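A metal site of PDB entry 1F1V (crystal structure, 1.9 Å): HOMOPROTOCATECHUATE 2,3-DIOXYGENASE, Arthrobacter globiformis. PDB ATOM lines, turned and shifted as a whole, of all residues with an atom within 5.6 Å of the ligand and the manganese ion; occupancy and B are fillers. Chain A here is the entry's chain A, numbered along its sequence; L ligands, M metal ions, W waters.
Water W1 bridges a ring nitrogen (NE2) of His 200 and the side-chain amide nitrogen (ND2) of Asn 157.
An oxygen (O2) of the ligand sits at hydrogen-bond distance from a ring nitrogen (ND1) of His 248, 2.5 Å away. O1 of the ligand is in salt-bridge range of NH1 of Arg 293 (3.0 Å). NH1 of Arg 243 is in salt-bridge range of O1 of the ligand. The backbone carbonyl oxygen of Arg 293 sits close to an oxygen (O2) of the ligand (2.8 Å). The side-chain hydroxyl of Tyr 257 sits close to an oxygen (O3) of the ligand (2.7 Å). NE2 of His 200 lies close to O4 of the ligand (3.3 Å).
The side-chain carboxylate (OE2) of Glu 267 sits at hydrogen-bond distance from the side-chain hydroxyl (OH) of Tyr 257 (3.2 Å). The side-chain hydroxyl (OH) of Tyr 257 sits close to a ring nitrogen (NE2) of His 248 (3.4 Å). The backbone NH (N) of Val 250 is in hydrogen-bond range of the backbone carbonyl oxygen (O) of Arg 292. O of Arg 293 sits close to ND1 of His 248, at 3.5 Å. A ring nitrogen (ND1) of His 155 lies close to a ring nitrogen (NE2) of His 200 (3.4 Å). N of Asn 157 is in hydrogen-bond range of O of His 214 (2.8 Å). The backbone carbonyl oxygen (O) of Arg 293 is in hydrogen-bond range of the backbone NH (N) of Gly 249 (3.0 Å). NH2 of Arg 243 lies within hydrogen-bond range of OH of Tyr 255, 3.2 Å away.
Residues that only touch the ligand: Asn 157 (3.97 Å), Trp 192 (3.4 Å), Val 250 (3.2 Å), Ser 251 (3.3 Å), Tyr 269 (3.6 Å) and Trp 304 (3.5 Å). 14 residues have an atom within 4 Å of the ligand: His 155, Asn 157, Trp 192, His 200, His 214, Arg 243, His 248, Val 250, Ser 251, Tyr 257, Glu 267, Tyr 269, Arg 293 and Trp 304.
The manganese ion is bound by an oxygen (O3) of the ligand (1.9 Å), the side-chain carboxylate (OE1) of Glu 267 (2.0 Å), a ring nitrogen (NE2) of His 155 (2.1 Å), an oxygen (O4) of the ligand (2.1 Å), a ring nitrogen (NE2) of His 214 (2.2 Å) and water W1 (2.3 Å). The manganese ion has six donor atoms within binding distance.
NE2 of His 200 touches the manganese ion (3.9 Å). Tyr 257 touches the manganese ion (OH to MN, 3.9 Å). Five residues have an atom within 4 Å of the manganese ion: His 155, His 200, His 214, Tyr 257 and Glu 267.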
ATOM      1  N   HIS A 155     -17.620   4.524 -29.791  1.00  0.00           N
ATOM      2  CA  HIS A 155     -17.529   3.208 -29.108  1.00  0.00           C
ATOM      3  C   HIS A 155     -18.877   2.549 -28.828  1.00  0.00           C
ATOM      4  O   HIS A 155     -19.980   3.142 -29.034  1.00  0.00           O
ATOM      5  CB  HIS A 155     -16.792   3.362 -27.752  1.00  0.00           C
ATOM      6  CG  HIS A 155     -17.530   4.230 -26.748  1.00  0.00           C
ATOM      7  ND1 HIS A 155     -17.243   5.574 -26.575  1.00  0.00           N
ATOM      8  CD2 HIS A 155     -18.454   3.933 -25.803  1.00  0.00           C
ATOM      9  CE1 HIS A 155     -17.952   6.056 -25.558  1.00  0.00           C
ATOM     10  NE2 HIS A 155     -18.689   5.071 -25.076  1.00  0.00           N
ATOM     11  N   ASN A 157     -20.805  -0.071 -25.710  1.00  0.00           N
ATOM     12  CA  ASN A 157     -20.635  -0.478 -24.329  1.00  0.00           C
ATOM     13  C   ASN A 157     -21.589  -1.724 -24.166  1.00  0.00           C
ATOM     14  O   ASN A 157     -22.761  -1.694 -24.576  1.00  0.00           O
ATOM     15  CB  ASN A 157     -21.014   0.620 -23.342  1.00  0.00           C
ATOM     16  CG  ASN A 157     -20.654   0.250 -21.917  1.00  0.00           C
ATOM     17  OD1 ASN A 157     -21.038  -0.834 -21.420  1.00  0.00           O
ATOM     18  ND2 ASN A 157     -19.885   1.114 -21.241  1.00  0.00           N
ATOM     19  N   TRP A 192     -12.415  -0.634 -20.023  1.00  0.00           N
ATOM     20  CA  TRP A 192     -12.503   0.159 -21.226  1.00  0.00           C
ATOM     21  C   TRP A 192     -11.402  -0.365 -22.152  1.00  0.00           C
ATOM     22  O   TRP A 192     -10.215  -0.335 -21.786  1.00  0.00           O
ATOM     23  CB  TRP A 192     -12.335   1.616 -20.845  1.00  0.00           C
ATOM     24  CG  TRP A 192     -13.626   2.170 -20.299  1.00  0.00           C
ATOM     25  CD1 TRP A 192     -14.522   3.027 -20.957  1.00  0.00           C
ATOM     26  CD2 TRP A 192     -14.181   1.943 -18.994  1.00  0.00           C
ATOM     27  NE1 TRP A 192     -15.589   3.327 -20.095  1.00  0.00           N
ATOM     28  CE2 TRP A 192     -15.394   2.674 -18.906  1.00  0.00           C
ATOM     29  CE3 TRP A 192     -13.765   1.195 -17.890  1.00  0.00           C
ATOM     30  CZ2 TRP A 192     -16.178   2.690 -17.751  1.00  0.00           C
ATOM     31  CZ3 TRP A 192     -14.554   1.205 -16.728  1.00  0.00           C
ATOM     32  CH2 TRP A 192     -15.749   1.947 -16.676  1.00  0.00           C
ATOM     33  N   HIS A 200     -11.462   4.044 -25.899  1.00  0.00           N
ATOM     34  CA  HIS A 200     -12.056   2.727 -26.186  1.00  0.00           C
ATOM     35  C   HIS A 200     -12.819   2.573 -27.443  1.00  0.00           C
ATOM     36  O   HIS A 200     -13.291   3.556 -27.985  1.00  0.00           O
ATOM     37  CB  HIS A 200     -12.956   2.239 -25.028  1.00  0.00           C
ATOM     38  CG  HIS A 200     -14.153   3.117 -24.705  1.00  0.00           C
ATOM     39  ND1 HIS A 200     -14.068   4.469 -24.517  1.00  0.00           N
ATOM     40  CD2 HIS A 200     -15.412   2.779 -24.293  1.00  0.00           C
ATOM     41  CE1 HIS A 200     -15.192   4.934 -23.988  1.00  0.00           C
ATOM     42  NE2 HIS A 200     -16.026   3.931 -23.836  1.00  0.00           N
ATOM     43  N   HIS A 214     -24.941   0.853 -24.569  1.00  0.00           N
ATOM     44  CA  HIS A 214     -25.069   2.026 -25.395  1.00  0.00           C
ATOM     45  C   HIS A 214     -24.072   2.051 -26.546  1.00  0.00           C
ATOM     46  O   HIS A 214     -23.078   1.300 -26.566  1.00  0.00           O
ATOM     47  CB  HIS A 214     -24.893   3.327 -24.577  1.00  0.00           C
ATOM     48  CG  HIS A 214     -23.549   3.502 -23.974  1.00  0.00           C
ATOM     49  ND1 HIS A 214     -23.244   3.078 -22.696  1.00  0.00           N
ATOM     50  CD2 HIS A 214     -22.432   4.128 -24.446  1.00  0.00           C
ATOM     51  CE1 HIS A 214     -22.004   3.441 -22.398  1.00  0.00           C
ATOM     52  NE2 HIS A 214     -21.487   4.075 -23.437  1.00  0.00           N
ATOM     53  N   ALA A 216     -21.951   5.111 -28.741  1.00  0.00           N
ATOM     54  CA  ALA A 216     -21.555   6.517 -28.493  1.00  0.00           C
ATOM     55  C   ALA A 216     -21.034   7.263 -29.709  1.00  0.00           C
ATOM     56  O   ALA A 216     -20.208   6.728 -30.512  1.00  0.00           O
ATOM     57  CB  ALA A 216     -20.454   6.559 -27.420  1.00  0.00           C
ATOM     58  N   ARG A 243     -29.271  10.685 -18.344  1.00  0.00           N
ATOM     59  CA  ARG A 243     -28.205  10.960 -17.413  1.00  0.00           C
ATOM     60  C   ARG A 243     -27.273  11.993 -18.019  1.00  0.00           C
ATOM     61  O   ARG A 243     -26.952  11.902 -19.220  1.00  0.00           O
ATOM     62  CB  ARG A 243     -27.432   9.652 -17.136  1.00  0.00           C
ATOM     63  CG  ARG A 243     -26.243   9.818 -16.242  1.00  0.00           C
ATOM     64  CD  ARG A 243     -25.480   8.513 -15.956  1.00  0.00           C
ATOM     65  NE  ARG A 243     -24.202   8.870 -15.362  1.00  0.00           N
ATOM     66  CZ  ARG A 243     -23.092   8.147 -15.405  1.00  0.00           C
ATOM     67  NH1 ARG A 243     -23.046   6.963 -16.001  1.00  0.00           N
ATOM     68  NH2 ARG A 243     -21.979   8.637 -14.881  1.00  0.00           N
ATOM     69  N   HIS A 248     -17.076  12.496 -17.025  1.00  0.00           N
ATOM     70  CA  HIS A 248     -16.748  11.132 -16.571  1.00  0.00           C
ATOM     71  C   HIS A 248     -15.388  11.176 -15.806  1.00  0.00           C
ATOM     72  O   HIS A 248     -14.461  11.902 -16.226  1.00  0.00           O
ATOM     73  CB  HIS A 248     -16.459  10.198 -17.768  1.00  0.00           C
ATOM     74  CG  HIS A 248     -17.666   9.694 -18.483  1.00  0.00           C
ATOM     75  ND1 HIS A 248     -18.690   9.027 -17.835  1.00  0.00           N
ATOM     76  CD2 HIS A 248     -17.999   9.717 -19.803  1.00  0.00           C
ATOM     77  CE1 HIS A 248     -19.597   8.674 -18.720  1.00  0.00           C
ATOM     78  NE2 HIS A 248     -19.202   9.073 -19.921  1.00  0.00           N
ATOM     79  N   GLY A 249     -15.238  10.365 -14.763  1.00  0.00           N
ATOM     80  CA  GLY A 249     -13.941  10.254 -14.111  1.00  0.00           C
ATOM     81  C   GLY A 249     -13.173   9.374 -15.099  1.00  0.00           C
ATOM     82  O   GLY A 249     -12.213   9.827 -15.728  1.00  0.00           O
ATOM     83  N   VAL A 250     -13.582   8.086 -15.220  1.00  0.00           N
ATOM     84  CA  VAL A 250     -12.982   7.157 -16.214  1.00  0.00           C
ATOM     85  C   VAL A 250     -13.189   7.783 -17.629  1.00  0.00           C
ATOM     86  O   VAL A 250     -14.318   8.186 -17.962  1.00  0.00           O
ATOM     87  CB  VAL A 250     -13.742   5.778 -16.215  1.00  0.00           C
ATOM     88  CG1 VAL A 250     -13.256   4.899 -17.409  1.00  0.00           C
ATOM     89  CG2 VAL A 250     -13.556   5.094 -14.878  1.00  0.00           C
ATOM     90  N   SER A 251     -12.126   7.865 -18.413  1.00  0.00           N
ATOM     91  CA  SER A 251     -12.106   8.422 -19.766  1.00  0.00           C
ATOM     92  C   SER A 251     -11.954   9.933 -19.818  1.00  0.00           C
ATOM     93  O   SER A 251     -11.425  10.462 -20.812  1.00  0.00           O
ATOM     94  CB  SER A 251     -13.368   8.017 -20.580  1.00  0.00           C
ATOM     95  OG  SER A 251     -14.470   8.918 -20.374  1.00  0.00           O
ATOM     96  N   TYR A 255     -20.006  14.132 -21.180  1.00  0.00           N
ATOM     97  CA  TYR A 255     -20.996  13.193 -21.699  1.00  0.00           C
ATOM     98  C   TYR A 255     -22.447  13.486 -21.516  1.00  0.00           C
ATOM     99  O   TYR A 255     -22.829  14.282 -20.608  1.00  0.00           O
ATOM    100  CB  TYR A 255     -20.766  11.795 -21.064  1.00  0.00           C
ATOM    101  CG  TYR A 255     -21.211  11.726 -19.607  1.00  0.00           C
ATOM    102  CD1 TYR A 255     -22.560  11.544 -19.275  1.00  0.00           C
ATOM    103  CD2 TYR A 255     -20.303  11.932 -18.569  1.00  0.00           C
ATOM    104  CE1 TYR A 255     -22.999  11.594 -17.943  1.00  0.00           C
ATOM    105  CE2 TYR A 255     -20.720  11.972 -17.243  1.00  0.00           C
ATOM    106  CZ  TYR A 255     -22.065  11.800 -16.931  1.00  0.00           C
ATOM    107  OH  TYR A 255     -22.464  11.753 -15.600  1.00  0.00           O
ATOM    108  N   TYR A 257     -26.298  11.021 -21.934  1.00  0.00           N
ATOM    109  CA  TYR A 257     -27.003   9.800 -22.336  1.00  0.00           C
ATOM    110  C   TYR A 257     -28.468  10.088 -22.588  1.00  0.00           C
ATOM    111  O   TYR A 257     -29.132  10.623 -21.688  1.00  0.00           O
ATOM    112  CB  TYR A 257     -26.944   8.722 -21.233  1.00  0.00           C
ATOM    113  CG  TYR A 257     -25.545   8.209 -21.001  1.00  0.00           C
ATOM    114  CD1 TYR A 257     -24.971   7.223 -21.837  1.00  0.00           C
ATOM    115  CD2 TYR A 257     -24.777   8.711 -19.941  1.00  0.00           C
ATOM    116  CE1 TYR A 257     -23.672   6.741 -21.584  1.00  0.00           C
ATOM    117  CE2 TYR A 257     -23.458   8.224 -19.707  1.00  0.00           C
ATOM    118  CZ  TYR A 257     -22.933   7.251 -20.525  1.00  0.00           C
ATOM    119  OH  TYR A 257     -21.655   6.803 -20.231  1.00  0.00           O
ATOM    120  N   GLU A 267     -25.046   7.579 -26.318  1.00  0.00           N
ATOM    121  CA  GLU A 267     -24.219   8.523 -25.563  1.00  0.00           C
ATOM    122  C   GLU A 267     -23.660   9.548 -26.541  1.00  0.00           C
ATOM    123  O   GLU A 267     -23.347   9.188 -27.679  1.00  0.00           O
ATOM    124  CB  GLU A 267     -23.055   7.824 -24.870  1.00  0.00           C
ATOM    125  CG  GLU A 267     -22.143   8.763 -24.097  1.00  0.00           C
ATOM    126  CD  GLU A 267     -21.000   8.030 -23.447  1.00  0.00           C
ATOM    127  OE1 GLU A 267     -20.751   6.842 -23.828  1.00  0.00           O
ATOM    128  OE2 GLU A 267     -20.357   8.626 -22.559  1.00  0.00           O
ATOM    129  N   TYR A 269     -20.603  12.199 -26.625  1.00  0.00           N
ATOM    130  CA  TYR A 269     -19.342  12.231 -25.886  1.00  0.00           C
ATOM    131  C   TYR A 269     -18.342  13.190 -26.513  1.00  0.00           C
ATOM    132  O   TYR A 269     -18.322  13.334 -27.717  1.00  0.00           O
ATOM    133  CB  TYR A 269     -18.837  10.781 -26.083  1.00  0.00           C
ATOM    134  CG  TYR A 269     -17.530  10.332 -25.557  1.00  0.00           C
ATOM    135  CD1 TYR A 269     -16.317  10.507 -26.285  1.00  0.00           C
ATOM    136  CD2 TYR A 269     -17.499   9.539 -24.383  1.00  0.00           C
ATOM    137  CE1 TYR A 269     -15.122   9.889 -25.847  1.00  0.00           C
ATOM    138  CE2 TYR A 269     -16.333   8.915 -23.943  1.00  0.00           C
ATOM    139  CZ  TYR A 269     -15.148   9.081 -24.655  1.00  0.00           C
ATOM    140  OH  TYR A 269     -14.049   8.400 -24.162  1.00  0.00           O
ATOM    141  N   ARG A 292     -15.278   8.057  -9.863  1.00  0.00           N
ATOM    142  CA  ARG A 292     -14.910   7.251 -11.015  1.00  0.00           C
ATOM    143  C   ARG A 292     -15.953   7.293 -12.125  1.00  0.00           C
ATOM    144  O   ARG A 292     -15.615   7.116 -13.293  1.00  0.00           O
ATOM    145  CB  ARG A 292     -14.645   5.788 -10.630  1.00  0.00           C
ATOM    146  CG  ARG A 292     -15.911   5.026 -10.262  1.00  0.00           C
ATOM    147  CD  ARG A 292     -15.627   3.716  -9.545  1.00  0.00           C
ATOM    148  NE  ARG A 292     -16.782   3.424  -8.730  1.00  0.00           N
ATOM    149  CZ  ARG A 292     -17.860   2.760  -9.142  1.00  0.00           C
ATOM    150  NH1 ARG A 292     -17.934   2.265 -10.375  1.00  0.00           N
ATOM    151  NH2 ARG A 292     -18.915   2.661  -8.334  1.00  0.00           N
ATOM    152  N   ARG A 293     -17.216   7.513 -11.795  1.00  0.00           N
ATOM    153  CA  ARG A 293     -18.209   7.508 -12.858  1.00  0.00           C
ATOM    154  C   ARG A 293     -18.415   8.958 -13.284  1.00  0.00           C
ATOM    155  O   ARG A 293     -18.086   9.357 -14.417  1.00  0.00           O
ATOM    156  CB  ARG A 293     -19.536   6.876 -12.374  1.00  0.00           C
ATOM    157  CG  ARG A 293     -19.474   5.343 -12.098  1.00  0.00           C
ATOM    158  CD  ARG A 293     -20.172   4.469 -13.191  1.00  0.00           C
ATOM    159  NE  ARG A 293     -19.935   3.005 -13.097  1.00  0.00           N
ATOM    160  CZ  ARG A 293     -19.723   2.225 -14.170  1.00  0.00           C
ATOM    161  NH1 ARG A 293     -19.730   2.769 -15.390  1.00  0.00           N
ATOM    162  NH2 ARG A 293     -19.492   0.912 -14.036  1.00  0.00           N
ATOM    163  N   ASP A 294     -18.916   9.732 -12.336  1.00  0.00           N
ATOM    164  CA  ASP A 294     -19.145  11.142 -12.541  1.00  0.00           C
ATOM    165  C   ASP A 294     -18.155  11.943 -11.653  1.00  0.00           C
ATOM    166  O   ASP A 294     -18.185  11.927 -10.415  1.00  0.00           O
ATOM    167  CB  ASP A 294     -20.607  11.452 -12.250  1.00  0.00           C
ATOM    168  CG  ASP A 294     -20.969  12.855 -12.593  1.00  0.00           C
ATOM    169  OD1 ASP A 294     -20.718  13.731 -11.712  1.00  0.00           O
ATOM    170  OD2 ASP A 294     -21.474  13.099 -13.722  1.00  0.00           O
ATOM    171  N   TRP A 304     -29.840   3.433 -15.397  1.00  0.00           N
ATOM    172  CA  TRP A 304     -28.594   3.355 -16.137  1.00  0.00           C
ATOM    173  C   TRP A 304     -27.894   2.004 -15.862  1.00  0.00           C
ATOM    174  O   TRP A 304     -27.168   1.501 -16.717  1.00  0.00           O
ATOM    175  CB  TRP A 304     -27.670   4.552 -15.748  1.00  0.00           C
ATOM    176  CG  TRP A 304     -26.527   4.784 -16.725  1.00  0.00           C
ATOM    177  CD1 TRP A 304     -26.538   5.598 -17.822  1.00  0.00           C
ATOM    178  CD2 TRP A 304     -25.243   4.169 -16.711  1.00  0.00           C
ATOM    179  NE1 TRP A 304     -25.329   5.553 -18.475  1.00  0.00           N
ATOM    180  CE2 TRP A 304     -24.509   4.671 -17.806  1.00  0.00           C
ATOM    181  CE3 TRP A 304     -24.628   3.239 -15.865  1.00  0.00           C
ATOM    182  CZ2 TRP A 304     -23.215   4.286 -18.094  1.00  0.00           C
ATOM    183  CZ3 TRP A 304     -23.334   2.840 -16.150  1.00  0.00           C
ATOM    184  CH2 TRP A 304     -22.636   3.362 -17.256  1.00  0.00           C
HETATM  185  C1  LIG L   1     -18.040   5.729 -18.107  1.00  0.00           C
HETATM  186  C2  LIG L   1     -19.090   5.269 -18.964  1.00  0.00           C
HETATM  187  C3  LIG L   1     -19.015   5.438 -20.359  1.00  0.00           C
HETATM  188  C4  LIG L   1     -17.838   6.062 -20.936  1.00  0.00           C
HETATM  189  C5  LIG L   1     -16.760   6.518 -20.091  1.00  0.00           C
HETATM  190  C6  LIG L   1     -16.863   6.339 -18.679  1.00  0.00           C
HETATM  191  C7  LIG L   1     -18.271   5.503 -16.668  1.00  0.00           C
HETATM  192  C8  LIG L   1     -19.420   6.292 -16.109  1.00  0.00           C
HETATM  193  O1  LIG L   1     -20.443   5.677 -15.750  1.00  0.00           O
HETATM  194  O2  LIG L   1     -19.500   7.535 -15.987  1.00  0.00           O
HETATM  195  O3  LIG L   1     -19.962   5.085 -21.349  1.00  0.00           O
HETATM  196  O4  LIG L   1     -17.925   6.145 -22.362  1.00  0.00           O
HETATM  197 MN    MN M   1     -19.675   5.271 -23.211  1.00  0.00          MN
HETATM  198  O   HOH W   1     -18.508   3.373 -22.545  1.00  0.00           O
